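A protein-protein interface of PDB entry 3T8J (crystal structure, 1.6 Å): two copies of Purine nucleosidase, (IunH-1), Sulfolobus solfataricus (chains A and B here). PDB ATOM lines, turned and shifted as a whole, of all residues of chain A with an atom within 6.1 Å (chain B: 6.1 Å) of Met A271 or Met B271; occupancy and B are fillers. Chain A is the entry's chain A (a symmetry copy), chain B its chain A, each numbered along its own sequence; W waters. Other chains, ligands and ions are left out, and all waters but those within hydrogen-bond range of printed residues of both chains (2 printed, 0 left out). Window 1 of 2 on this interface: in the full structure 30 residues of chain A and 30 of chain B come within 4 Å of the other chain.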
ATOM      1  N   ALA A 150      30.815   6.157 -16.406  1.00  0.00           N
ATOM      2  CA  ALA A 150      30.581   7.177 -15.388  1.00  0.00           C
ATOM      3  C   ALA A 150      30.575   6.448 -14.049  1.00  0.00           C
ATOM      4  O   ALA A 150      29.638   5.730 -13.698  1.00  0.00           O
ATOM      5  CB  ALA A 150      29.269   7.937 -15.659  1.00  0.00           C
ATOM      6  N   GLY A 153      28.159   7.751 -11.529  1.00  0.00           N
ATOM      7  CA  GLY A 153      26.835   7.927 -12.120  1.00  0.00           C
ATOM      8  C   GLY A 153      26.511   9.338 -12.593  1.00  0.00           C
ATOM      9  O   GLY A 153      25.342   9.706 -12.581  1.00  0.00           O
ATOM     10  N   VAL A 160      22.779   9.176 -15.882  1.00  0.00           N
ATOM     11  CA  VAL A 160      23.651   8.238 -15.169  1.00  0.00           C
ATOM     12  C   VAL A 160      24.633   7.423 -16.032  1.00  0.00           C
ATOM     13  O   VAL A 160      25.451   6.683 -15.457  1.00  0.00           O
ATOM     14  CB  VAL A 160      22.807   7.258 -14.306  1.00  0.00           C
ATOM     15  CG1 VAL A 160      22.081   7.998 -13.164  1.00  0.00           C
ATOM     16  CG2 VAL A 160      21.820   6.473 -15.135  1.00  0.00           C
ATOM     17  N   ALA A 161      24.561   7.538 -17.355  1.00  0.00           N
ATOM     18  CA  ALA A 161      25.402   6.767 -18.275  1.00  0.00           C
ATOM     19  C   ALA A 161      26.195   7.663 -19.234  1.00  0.00           C
ATOM     20  O   ALA A 161      25.713   8.754 -19.654  1.00  0.00           O
ATOM     21  CB  ALA A 161      24.564   5.745 -19.062  1.00  0.00           C
ATOM     22  N   GLU A 162      27.360   7.179 -19.609  1.00  0.00           N
ATOM     23  CA  GLU A 162      28.261   7.791 -20.566  1.00  0.00           C
ATOM     24  C   GLU A 162      27.998   7.242 -21.981  1.00  0.00           C
ATOM     25  O   GLU A 162      27.670   6.071 -22.179  1.00  0.00           O
ATOM     26  CB  GLU A 162      29.709   7.559 -20.125  1.00  0.00           C
ATOM     27  CG  GLU A 162      30.764   8.131 -21.022  1.00  0.00           C
ATOM     28  CD  GLU A 162      31.057   7.258 -22.220  1.00  0.00           C
ATOM     29  OE1 GLU A 162      30.959   6.001 -22.100  1.00  0.00           O
ATOM     30  OE2 GLU A 162      31.425   7.824 -23.272  1.00  0.00           O
ATOM     31  N   ILE A 165      29.606   3.769 -23.797  1.00  0.00           N
ATOM     32  CA  ILE A 165      29.063   2.526 -23.238  1.00  0.00           C
ATOM     33  C   ILE A 165      27.567   2.401 -23.535  1.00  0.00           C
ATOM     34  O   ILE A 165      27.075   1.331 -23.927  1.00  0.00           O
ATOM     35  CB  ILE A 165      29.320   2.426 -21.719  1.00  0.00           C
ATOM     36  CG1 ILE A 165      30.812   2.616 -21.395  1.00  0.00           C
ATOM     37  CG2 ILE A 165      28.791   1.067 -21.122  1.00  0.00           C
ATOM     38  CD1 ILE A 165      31.737   1.580 -22.048  1.00  0.00           C
ATOM     39  N   TRP A 166      26.816   3.504 -23.373  1.00  0.00           N
ATOM     40  CA  TRP A 166      25.370   3.500 -23.612  1.00  0.00           C
ATOM     41  C   TRP A 166      24.995   3.120 -25.082  1.00  0.00           C
ATOM     42  O   TRP A 166      23.999   2.427 -25.307  1.00  0.00           O
ATOM     43  CB  TRP A 166      24.793   4.899 -23.271  1.00  0.00           C
ATOM     44  CG  TRP A 166      23.327   5.027 -23.519  1.00  0.00           C
ATOM     45  CD1 TRP A 166      22.294   4.767 -22.643  1.00  0.00           C
ATOM     46  CD2 TRP A 166      22.707   5.469 -24.734  1.00  0.00           C
ATOM     47  NE1 TRP A 166      21.076   4.988 -23.248  1.00  0.00           N
ATOM     48  CE2 TRP A 166      21.307   5.412 -24.538  1.00  0.00           C
ATOM     49  CE3 TRP A 166      23.201   5.882 -25.985  1.00  0.00           C
ATOM     50  CZ2 TRP A 166      20.405   5.769 -25.533  1.00  0.00           C
ATOM     51  CZ3 TRP A 166      22.295   6.235 -26.962  1.00  0.00           C
ATOM     52  CH2 TRP A 166      20.915   6.170 -26.732  1.00  0.00           C
ATOM     53  N   VAL A 260      30.795  -3.807 -13.833  1.00  0.00           N
ATOM     54  CA  VAL A 260      29.685  -4.492 -14.470  1.00  0.00           C
ATOM     55  C   VAL A 260      29.011  -3.490 -15.419  1.00  0.00           C
ATOM     56  O   VAL A 260      28.838  -2.344 -15.014  1.00  0.00           O
ATOM     57  CB  VAL A 260      28.663  -4.974 -13.471  1.00  0.00           C
ATOM     58  CG1 VAL A 260      27.462  -5.609 -14.173  1.00  0.00           C
ATOM     59  CG2 VAL A 260      29.313  -6.045 -12.541  1.00  0.00           C
ATOM     60  N   ILE A 261      28.739  -3.937 -16.648  1.00  0.00           N
ATOM     61  CA  ILE A 261      28.025  -3.088 -17.633  1.00  0.00           C
ATOM     62  C   ILE A 261      26.551  -3.442 -17.591  1.00  0.00           C
ATOM     63  O   ILE A 261      26.161  -4.604 -17.758  1.00  0.00           O
ATOM     64  CB  ILE A 261      28.548  -3.353 -19.036  1.00  0.00           C
ATOM     65  CG1 ILE A 261      30.067  -3.220 -19.134  1.00  0.00           C
ATOM     66  CG2 ILE A 261      27.818  -2.425 -20.051  1.00  0.00           C
ATOM     67  CD1 ILE A 261      30.613  -1.828 -18.762  1.00  0.00           C
ATOM     68  N   ASP A 262      25.704  -2.431 -17.422  1.00  0.00           N
ATOM     69  CA  ASP A 262      24.245  -2.623 -17.534  1.00  0.00           C
ATOM     70  C   ASP A 262      23.855  -2.631 -19.027  1.00  0.00           C
ATOM     71  O   ASP A 262      24.034  -1.615 -19.724  1.00  0.00           O
ATOM     72  CB  ASP A 262      23.489  -1.534 -16.786  1.00  0.00           C
ATOM     73  CG  ASP A 262      21.975  -1.727 -16.833  1.00  0.00           C
ATOM     74  OD1 ASP A 262      21.411  -1.926 -17.938  1.00  0.00           O
ATOM     75  OD2 ASP A 262      21.331  -1.652 -15.755  1.00  0.00           O
ATOM     76  N   ASN A 263      23.463  -3.805 -19.538  1.00  0.00           N
ATOM     77  CA  ASN A 263      23.065  -3.962 -20.944  1.00  0.00           C
ATOM     78  C   ASN A 263      21.569  -4.219 -21.096  1.00  0.00           C
ATOM     79  O   ASN A 263      21.127  -4.865 -22.050  1.00  0.00           O
ATOM     80  CB  ASN A 263      23.899  -5.038 -21.657  1.00  0.00           C
ATOM     81  CG  ASN A 263      23.582  -6.442 -21.171  1.00  0.00           C
ATOM     82  OD1 ASN A 263      23.298  -6.653 -19.968  1.00  0.00           O
ATOM     83  ND2 ASN A 263      23.650  -7.422 -22.082  1.00  0.00           N
ATOM     84  N   ILE A 267      15.992   2.008 -17.603  1.00  0.00           N
ATOM     85  CA  ILE A 267      16.517   3.331 -17.343  1.00  0.00           C
ATOM     86  C   ILE A 267      18.046   3.390 -17.054  1.00  0.00           C
ATOM     87  O   ILE A 267      18.687   4.394 -17.312  1.00  0.00           O
ATOM     88  CB  ILE A 267      15.688   3.986 -16.205  1.00  0.00           C
ATOM     89  CG1 ILE A 267      15.807   5.489 -16.279  1.00  0.00           C
ATOM     90  CG2 ILE A 267      16.023   3.398 -14.842  1.00  0.00           C
ATOM     91  CD1 ILE A 267      14.739   6.188 -15.447  1.00  0.00           C
ATOM     92  N   THR A 268      18.597   2.296 -16.505  1.00  0.00           N
ATOM     93  CA  THR A 268      19.991   2.163 -16.132  1.00  0.00           C
ATOM     94  C   THR A 268      20.887   1.687 -17.290  1.00  0.00           C
ATOM     95  O   THR A 268      22.093   1.476 -17.109  1.00  0.00           O
ATOM     96  CB  THR A 268      20.109   1.149 -14.967  1.00  0.00           C
ATOM     97  OG1 THR A 268      19.323   0.002 -15.304  1.00  0.00           O
ATOM     98  CG2 THR A 268      19.618   1.778 -13.654  1.00  0.00           C
ATOM     99  N   ARG A 269      20.322   1.564 -18.499  1.00  0.00           N
ATOM    100  CA  ARG A 269      21.087   1.164 -19.670  1.00  0.00           C
ATOM    101  C   ARG A 269      22.408   1.913 -19.751  1.00  0.00           C
ATOM    102  O   ARG A 269      22.441   3.144 -19.678  1.00  0.00           O
ATOM    103  CB  ARG A 269      20.288   1.434 -20.956  1.00  0.00           C
ATOM    104  CG  ARG A 269      21.087   1.235 -22.243  1.00  0.00           C
ATOM    105  CD  ARG A 269      20.308   1.585 -23.518  1.00  0.00           C
ATOM    106  NE  ARG A 269      21.183   1.771 -24.663  1.00  0.00           N
ATOM    107  CZ  ARG A 269      20.773   1.937 -25.914  1.00  0.00           C
ATOM    108  NH1 ARG A 269      19.481   1.863 -26.179  1.00  0.00           N
ATOM    109  NH2 ARG A 269      21.652   2.134 -26.894  1.00  0.00           N
ATOM    110  N   GLY A 270      23.492   1.172 -19.966  1.00  0.00           N
ATOM    111  CA  GLY A 270      24.785   1.788 -20.198  1.00  0.00           C
ATOM    112  C   GLY A 270      25.584   2.200 -18.992  1.00  0.00           C
ATOM    113  O   GLY A 270      26.720   2.650 -19.149  1.00  0.00           O
ATOM    114  N   MET A 271      25.036   2.007 -17.791  1.00  0.00           N
ATOM    115  CA  MET A 271      25.796   2.303 -16.579  1.00  0.00           C
ATOM    116  C   MET A 271      26.987   1.374 -16.414  1.00  0.00           C
ATOM    117  O   MET A 271      26.952   0.199 -16.808  1.00  0.00           O
ATOM    118  CB  MET A 271      24.936   2.215 -15.315  1.00  0.00           C
ATOM    119  CG  MET A 271      23.890   3.330 -15.194  1.00  0.00           C
ATOM    120  SD  MET A 271      23.086   3.427 -13.596  1.00  0.00           S
ATOM    121  CE  MET A 271      24.368   4.162 -12.668  1.00  0.00           C
ATOM    122  N   THR A 272      28.060   1.960 -15.914  1.00  0.00           N
ATOM    123  CA  THR A 272      29.247   1.203 -15.431  1.00  0.00           C
ATOM    124  C   THR A 272      29.168   1.151 -13.900  1.00  0.00           C
ATOM    125  O   THR A 272      29.362   2.168 -13.209  1.00  0.00           O
ATOM    126  CB  THR A 272      30.549   1.877 -15.880  1.00  0.00           C
ATOM    127  OG1 THR A 272      30.532   3.256 -15.481  1.00  0.00           O
ATOM    128  CG2 THR A 272      30.739   1.790 -17.402  1.00  0.00           C
ATOM    129  N   LEU A 273      28.864  -0.042 -13.377  1.00  0.00           N
ATOM    130  CA  LEU A 273      28.637  -0.278 -11.939  1.00  0.00           C
ATOM    131  C   LEU A 273      29.930  -0.857 -11.353  1.00  0.00           C
ATOM    132  O   LEU A 273      30.338  -1.927 -11.761  1.00  0.00           O
ATOM    133  CB  LEU A 273      27.476  -1.250 -11.773  1.00  0.00           C
ATOM    134  CG  LEU A 273      26.210  -0.796 -12.548  1.00  0.00           C
ATOM    135  CD1 LEU A 273      25.257  -1.953 -12.767  1.00  0.00           C
ATOM    136  CD2 LEU A 273      25.543   0.451 -11.932  1.00  0.00           C
ATOM    137  N   ALA B 150      22.166   6.811  -2.547  1.00  0.00           N
ATOM    138  CA  ALA B 150      23.562   7.056  -2.899  1.00  0.00           C
ATOM    139  C   ALA B 150      23.542   7.756  -4.253  1.00  0.00           C
ATOM    140  O   ALA B 150      23.270   7.159  -5.296  1.00  0.00           O
ATOM    141  CB  ALA B 150      24.364   5.741  -2.920  1.00  0.00           C
ATOM    142  N   GLY B 153      26.312   6.838  -6.570  1.00  0.00           N
ATOM    143  CA  GLY B 153      26.466   5.389  -6.649  1.00  0.00           C
ATOM    144  C   GLY B 153      27.538   4.793  -5.747  1.00  0.00           C
ATOM    145  O   GLY B 153      28.101   3.764  -6.108  1.00  0.00           O
ATOM    146  N   VAL B 160      26.660  -0.063  -5.099  1.00  0.00           N
ATOM    147  CA  VAL B 160      25.995   1.099  -5.693  1.00  0.00           C
ATOM    148  C   VAL B 160      24.695   1.568  -5.013  1.00  0.00           C
ATOM    149  O   VAL B 160      24.148   2.605  -5.431  1.00  0.00           O
ATOM    150  CB  VAL B 160      25.712   0.852  -7.202  1.00  0.00           C
ATOM    151  CG1 VAL B 160      27.021   0.748  -8.010  1.00  0.00           C
ATOM    152  CG2 VAL B 160      24.854  -0.370  -7.429  1.00  0.00           C
ATOM    153  N   ALA B 161      24.205   0.843  -4.011  1.00  0.00           N
ATOM    154  CA  ALA B 161      22.948   1.160  -3.330  1.00  0.00           C
ATOM    155  C   ALA B 161      23.124   1.319  -1.815  1.00  0.00           C
ATOM    156  O   ALA B 161      23.977   0.632  -1.183  1.00  0.00           O
ATOM    157  CB  ALA B 161      21.874   0.101  -3.638  1.00  0.00           C
ATOM    158  N   GLU B 162      22.297   2.171  -1.247  1.00  0.00           N
ATOM    159  CA  GLU B 162      22.207   2.442   0.174  1.00  0.00           C
ATOM    160  C   GLU B 162      21.140   1.542   0.828  1.00  0.00           C
ATOM    161  O   GLU B 162      20.102   1.227   0.244  1.00  0.00           O
ATOM    162  CB  GLU B 162      21.911   3.928   0.394  1.00  0.00           C
ATOM    163  CG  GLU B 162      21.782   4.364   1.821  1.00  0.00           C
ATOM    164  CD  GLU B 162      20.420   4.073   2.407  1.00  0.00           C
ATOM    165  OE1 GLU B 162      19.406   4.119   1.650  1.00  0.00           O
ATOM    166  OE2 GLU B 162      20.356   3.838   3.633  1.00  0.00           O
ATOM    167  N   ILE B 165      16.975   2.233   1.180  1.00  0.00           N
ATOM    168  CA  ILE B 165      16.264   2.110  -0.098  1.00  0.00           C
ATOM    169  C   ILE B 165      16.325   0.674  -0.622  1.00  0.00           C
ATOM    170  O   ILE B 165      15.320   0.114  -1.088  1.00  0.00           O
ATOM    171  CB  ILE B 165      16.817   3.093  -1.153  1.00  0.00           C
ATOM    172  CG1 ILE B 165      16.824   4.534  -0.618  1.00  0.00           C
ATOM    173  CG2 ILE B 165      16.020   3.007  -2.509  1.00  0.00           C
ATOM    174  CD1 ILE B 165      15.440   5.071  -0.228  1.00  0.00           C
ATOM    175  N   TRP B 166      17.508   0.041  -0.536  1.00  0.00           N
ATOM    176  CA  TRP B 166      17.690  -1.330  -1.022  1.00  0.00           C
ATOM    177  C   TRP B 166      16.768  -2.362  -0.295  1.00  0.00           C
ATOM    178  O   TRP B 166      16.268  -3.298  -0.926  1.00  0.00           O
ATOM    179  CB  TRP B 166      19.176  -1.741  -0.842  1.00  0.00           C
ATOM    180  CG  TRP B 166      19.473  -3.141  -1.264  1.00  0.00           C
ATOM    181  CD1 TRP B 166      19.857  -3.587  -2.511  1.00  0.00           C
ATOM    182  CD2 TRP B 166      19.429  -4.306  -0.429  1.00  0.00           C
ATOM    183  NE1 TRP B 166      20.022  -4.954  -2.510  1.00  0.00           N
ATOM    184  CE2 TRP B 166      19.754  -5.419  -1.241  1.00  0.00           C
ATOM    185  CE3 TRP B 166      19.115  -4.523   0.925  1.00  0.00           C
ATOM    186  CZ2 TRP B 166      19.794  -6.714  -0.740  1.00  0.00           C
ATOM    187  CZ3 TRP B 166      19.161  -5.812   1.409  1.00  0.00           C
ATOM    188  CH2 TRP B 166      19.491  -6.890   0.578  1.00  0.00           C
ATOM    189  N   VAL B 260      14.711   8.638  -9.400  1.00  0.00           N
ATOM    190  CA  VAL B 260      14.053   7.399  -9.776  1.00  0.00           C
ATOM    191  C   VAL B 260      14.626   6.288  -8.885  1.00  0.00           C
ATOM    192  O   VAL B 260      15.839   6.274  -8.694  1.00  0.00           O
ATOM    193  CB  VAL B 260      14.300   7.037 -11.218  1.00  0.00           C
ATOM    194  CG1 VAL B 260      13.674   5.684 -11.562  1.00  0.00           C
ATOM    195  CG2 VAL B 260      13.663   8.123 -12.141  1.00  0.00           C
ATOM    196  N   ILE B 261      13.734   5.467  -8.321  1.00  0.00           N
ATOM    197  CA  ILE B 261      14.166   4.311  -7.498  1.00  0.00           C
ATOM    198  C   ILE B 261      14.180   3.077  -8.377  1.00  0.00           C
ATOM    199  O   ILE B 261      13.176   2.722  -9.007  1.00  0.00           O
ATOM    200  CB  ILE B 261      13.191   4.084  -6.354  1.00  0.00           C
ATOM    201  CG1 ILE B 261      12.952   5.344  -5.523  1.00  0.00           C
ATOM    202  CG2 ILE B 261      13.681   2.895  -5.477  1.00  0.00           C
ATOM    203  CD1 ILE B 261      14.216   5.922  -4.860  1.00  0.00           C
ATOM    204  N   ASP B 262      15.306   2.368  -8.386  1.00  0.00           N
ATOM    205  CA  ASP B 262      15.386   1.060  -9.063  1.00  0.00           C
ATOM    206  C   ASP B 262      14.778  -0.019  -8.143  1.00  0.00           C
ATOM    207  O   ASP B 262      15.305  -0.267  -7.042  1.00  0.00           O
ATOM    208  CB  ASP B 262      16.825   0.714  -9.421  1.00  0.00           C
ATOM    209  CG  ASP B 262      16.945  -0.610 -10.171  1.00  0.00           C
ATOM    210  OD1 ASP B 262      16.384  -1.635  -9.711  1.00  0.00           O
ATOM    211  OD2 ASP B 262      17.633  -0.637 -11.224  1.00  0.00           O
ATOM    212  N   ASN B 263      13.608  -0.545  -8.525  1.00  0.00           N
ATOM    213  CA  ASN B 263      12.913  -1.578  -7.746  1.00  0.00           C
ATOM    214  C   ASN B 263      12.926  -2.935  -8.443  1.00  0.00           C
ATOM    215  O   ASN B 263      12.021  -3.754  -8.259  1.00  0.00           O
ATOM    216  CB  ASN B 263      11.485  -1.147  -7.372  1.00  0.00           C
ATOM    217  CG  ASN B 263      10.555  -1.102  -8.573  1.00  0.00           C
ATOM    218  OD1 ASN B 263      10.978  -0.739  -9.696  1.00  0.00           O
ATOM    219  ND2 ASN B 263       9.277  -1.439  -8.355  1.00  0.00           N
ATOM    220  N   ILE B 267      21.051  -6.388 -10.477  1.00  0.00           N
ATOM    221  CA  ILE B 267      22.208  -5.880  -9.773  1.00  0.00           C
ATOM    222  C   ILE B 267      22.080  -4.416  -9.261  1.00  0.00           C
ATOM    223  O   ILE B 267      22.700  -4.046  -8.279  1.00  0.00           O
ATOM    224  CB  ILE B 267      23.463  -6.072 -10.667  1.00  0.00           C
ATOM    225  CG1 ILE B 267      24.707  -6.091  -9.813  1.00  0.00           C
ATOM    226  CG2 ILE B 267      23.507  -5.071 -11.813  1.00  0.00           C
ATOM    227  CD1 ILE B 267      25.911  -6.643 -10.567  1.00  0.00           C
ATOM    228  N   THR B 268      21.269  -3.603  -9.957  1.00  0.00           N
ATOM    229  CA  THR B 268      21.039  -2.203  -9.664  1.00  0.00           C
ATOM    230  C   THR B 268      19.916  -1.975  -8.636  1.00  0.00           C
ATOM    231  O   THR B 268      19.570  -0.828  -8.325  1.00  0.00           O
ATOM    232  CB  THR B 268      20.668  -1.465 -10.975  1.00  0.00           C
ATOM    233  OG1 THR B 268      19.681  -2.248 -11.652  1.00  0.00           O
ATOM    234  CG2 THR B 268      21.911  -1.275 -11.856  1.00  0.00           C
ATOM    235  N   ARG B 269      19.374  -3.057  -8.062  1.00  0.00           N
ATOM    236  CA  ARG B 269      18.338  -2.952  -7.046  1.00  0.00           C
ATOM    237  C   ARG B 269      18.680  -1.890  -6.012  1.00  0.00           C
ATOM    238  O   ARG B 269      19.774  -1.895  -5.440  1.00  0.00           O
ATOM    239  CB  ARG B 269      18.148  -4.298  -6.325  1.00  0.00           C
ATOM    240  CG  ARG B 269      17.226  -4.233  -5.110  1.00  0.00           C
ATOM    241  CD  ARG B 269      17.107  -5.560  -4.349  1.00  0.00           C
ATOM    242  NE  ARG B 269      16.567  -5.381  -3.011  1.00  0.00           N
ATOM    243  CZ  ARG B 269      16.226  -6.366  -2.191  1.00  0.00           C
ATOM    244  NH1 ARG B 269      16.304  -7.612  -2.621  1.00  0.00           N
ATOM    245  NH2 ARG B 269      15.770  -6.102  -0.969  1.00  0.00           N
ATOM    246  N   GLY B 270      17.719  -1.015  -5.727  1.00  0.00           N
ATOM    247  CA  GLY B 270      17.883  -0.045  -4.660  1.00  0.00           C
ATOM    248  C   GLY B 270      18.626   1.221  -4.984  1.00  0.00           C
ATOM    249  O   GLY B 270      18.713   2.103  -4.126  1.00  0.00           O
ATOM    250  N   MET B 271      19.119   1.354  -6.216  1.00  0.00           N
ATOM    251  CA  MET B 271      19.772   2.596  -6.618  1.00  0.00           C
ATOM    252  C   MET B 271      18.800   3.763  -6.658  1.00  0.00           C
ATOM    253  O   MET B 271      17.609   3.604  -6.965  1.00  0.00           O
ATOM    254  CB  MET B 271      20.448   2.483  -7.989  1.00  0.00           C
ATOM    255  CG  MET B 271      21.682   1.574  -8.001  1.00  0.00           C
ATOM    256  SD  MET B 271      22.658   1.665  -9.500  1.00  0.00           S
ATOM    257  CE  MET B 271      23.457   3.193  -9.237  1.00  0.00           C
ATOM    258  N   THR B 272      19.316   4.907  -6.247  1.00  0.00           N
ATOM    259  CA  THR B 272      18.639   6.218  -6.440  1.00  0.00           C
ATOM    260  C   THR B 272      19.308   6.913  -7.633  1.00  0.00           C
ATOM    261  O   THR B 272      20.464   7.366  -7.551  1.00  0.00           O
ATOM    262  CB  THR B 272      18.752   7.085  -5.179  1.00  0.00           C
ATOM    263  OG1 THR B 272      20.132   7.190  -4.798  1.00  0.00           O
ATOM    264  CG2 THR B 272      17.944   6.500  -4.011  1.00  0.00           C
ATOM    265  N   LEU B 273      18.574   6.977  -8.749  1.00  0.00           N
ATOM    266  CA  LEU B 273      19.071   7.507 -10.033  1.00  0.00           C
ATOM    267  C   LEU B 273      18.574   8.951 -10.163  1.00  0.00           C
ATOM    268  O   LEU B 273      17.377   9.163 -10.207  1.00  0.00           O
ATOM    269  CB  LEU B 273      18.542   6.639 -11.167  1.00  0.00           C
ATOM    270  CG  LEU B 273      18.840   5.132 -10.946  1.00  0.00           C
ATOM    271  CD1 LEU B 273      17.932   4.263 -11.793  1.00  0.00           C
ATOM    272  CD2 LEU B 273      20.338   4.788 -11.087  1.00  0.00           C
HETATM  273  O   HOH W   1      20.099  -3.433 -14.176  1.00  0.00           O
HETATM  274  O   HOH W   2      17.060  -0.820 -13.836  1.00  0.00           O
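The backbone carbonyl oxygen (O) of Val B260 lies within hydrogen-bond range of the backbone NH (N) of Leu B273 (2.8 Å). The backbone NH (N) of Gly B270 sits at hydrogen-bond distance from the backbone carbonyl oxygen (O) of Asp B262 (2.8 Å). O of Met B271 sits at hydrogen-bond distance from N of Asp B262. The backbone NH of Leu A273 lies within hydrogen-bond range of the backbone carbonyl oxygen of Val A260 (2.8 Å). The side-chain carboxylate of Asp A262 lies within hydrogen-bond range of the side-chain hydroxyl of Thr A268 (2.6 Å). The backbone carbonyl oxygen (O) of Met A271 lies within hydrogen-bond range of the backbone NH (N) of Asp A262 (3.0 Å).
Ile B267 touches Val A260. Thr B268 touches Asp A262. Ile A267 touches Val B260. Ile A267 touches Leu B273 (CG2 to CD1, 3.7 Å). Thr A268 touches Asp B262. Thr A268 touches Leu B273. SD of Met A271 touches CD2 of Leu B273, 3.96 Å away. CD1 of Leu A273 touches CG2 of Ile B267, at 3.7 Å. Leu A273 touches Thr B268. Leu A273 touches Met B271.
Of the printed residues of chain B, Asp A262 touches Thr B268 (3.96 Å). Asn A263 touches none of the printed residues of chain B. Of the printed residues of chain B, Ile A267 touches Val B260 and Leu B273. Of chain B, only Met B271 (3.7 Å) and Leu B273 (3.96 Å) come within 4 Å of Met A271. Printed residues of chain B within 4 Å of Leu A273: Ile B267, Thr B268 and Met B271. Trp B166 touches none of the printed residues of chain A. Printed residues of chain A within 4 Å of Asp B262: Thr A268 (3.96 Å). Printed residues of chain A within 4 Å of Ile B267: Val A260 (3.98 Å) and Leu A273 (3.7 Å). The nearest residue of chain B that does not touch Met A271 is Thr B268 (5.1 Å). The nearest residue of chain A that does not touch Met B271 is Thr A268 (5.1 Å).
Of the 18 printed residues of chain B, 6 touch a printed residue of chain A. Hydrophobic or aromatic side chains of chain B within 4 Å of the printed part of chain A: Val B260, Ile B267, Met B271 and Leu B273. Along chain B the printed residues that touch a printed residue of chain A span positions 260 to 273. Among the printed residues, 11 pairs touch across the chains. Among the printed residues, no Asp or Glu carboxylate lies within 4 Å of a Lys or Arg side-chain nitrogen of the other chain.
Val A260 touches Ile B267, and with the chains exchanged Ile A267 touches Val B260. Asp A262 touches Thr B268, and with the chains exchanged Thr A268 touches Asp B262. Met B271 touches its own counterpart, Met A271. Met A271 touches Leu B273, and with the chains exchanged Leu A273 touches Met B271. Of the 11 pairs that touch across the chains among the printed residues, 11 have their exchanged pair printed and touching as well.
Water W1 bridges the side-chain carboxylate of Asp A262 and the side-chain hydroxyl of Thr B268. Water W2 bridges the side-chain carboxylate of Asp B262 (2.7 Å) and the side-chain hydroxyl of Thr A268 (2.8 Å).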
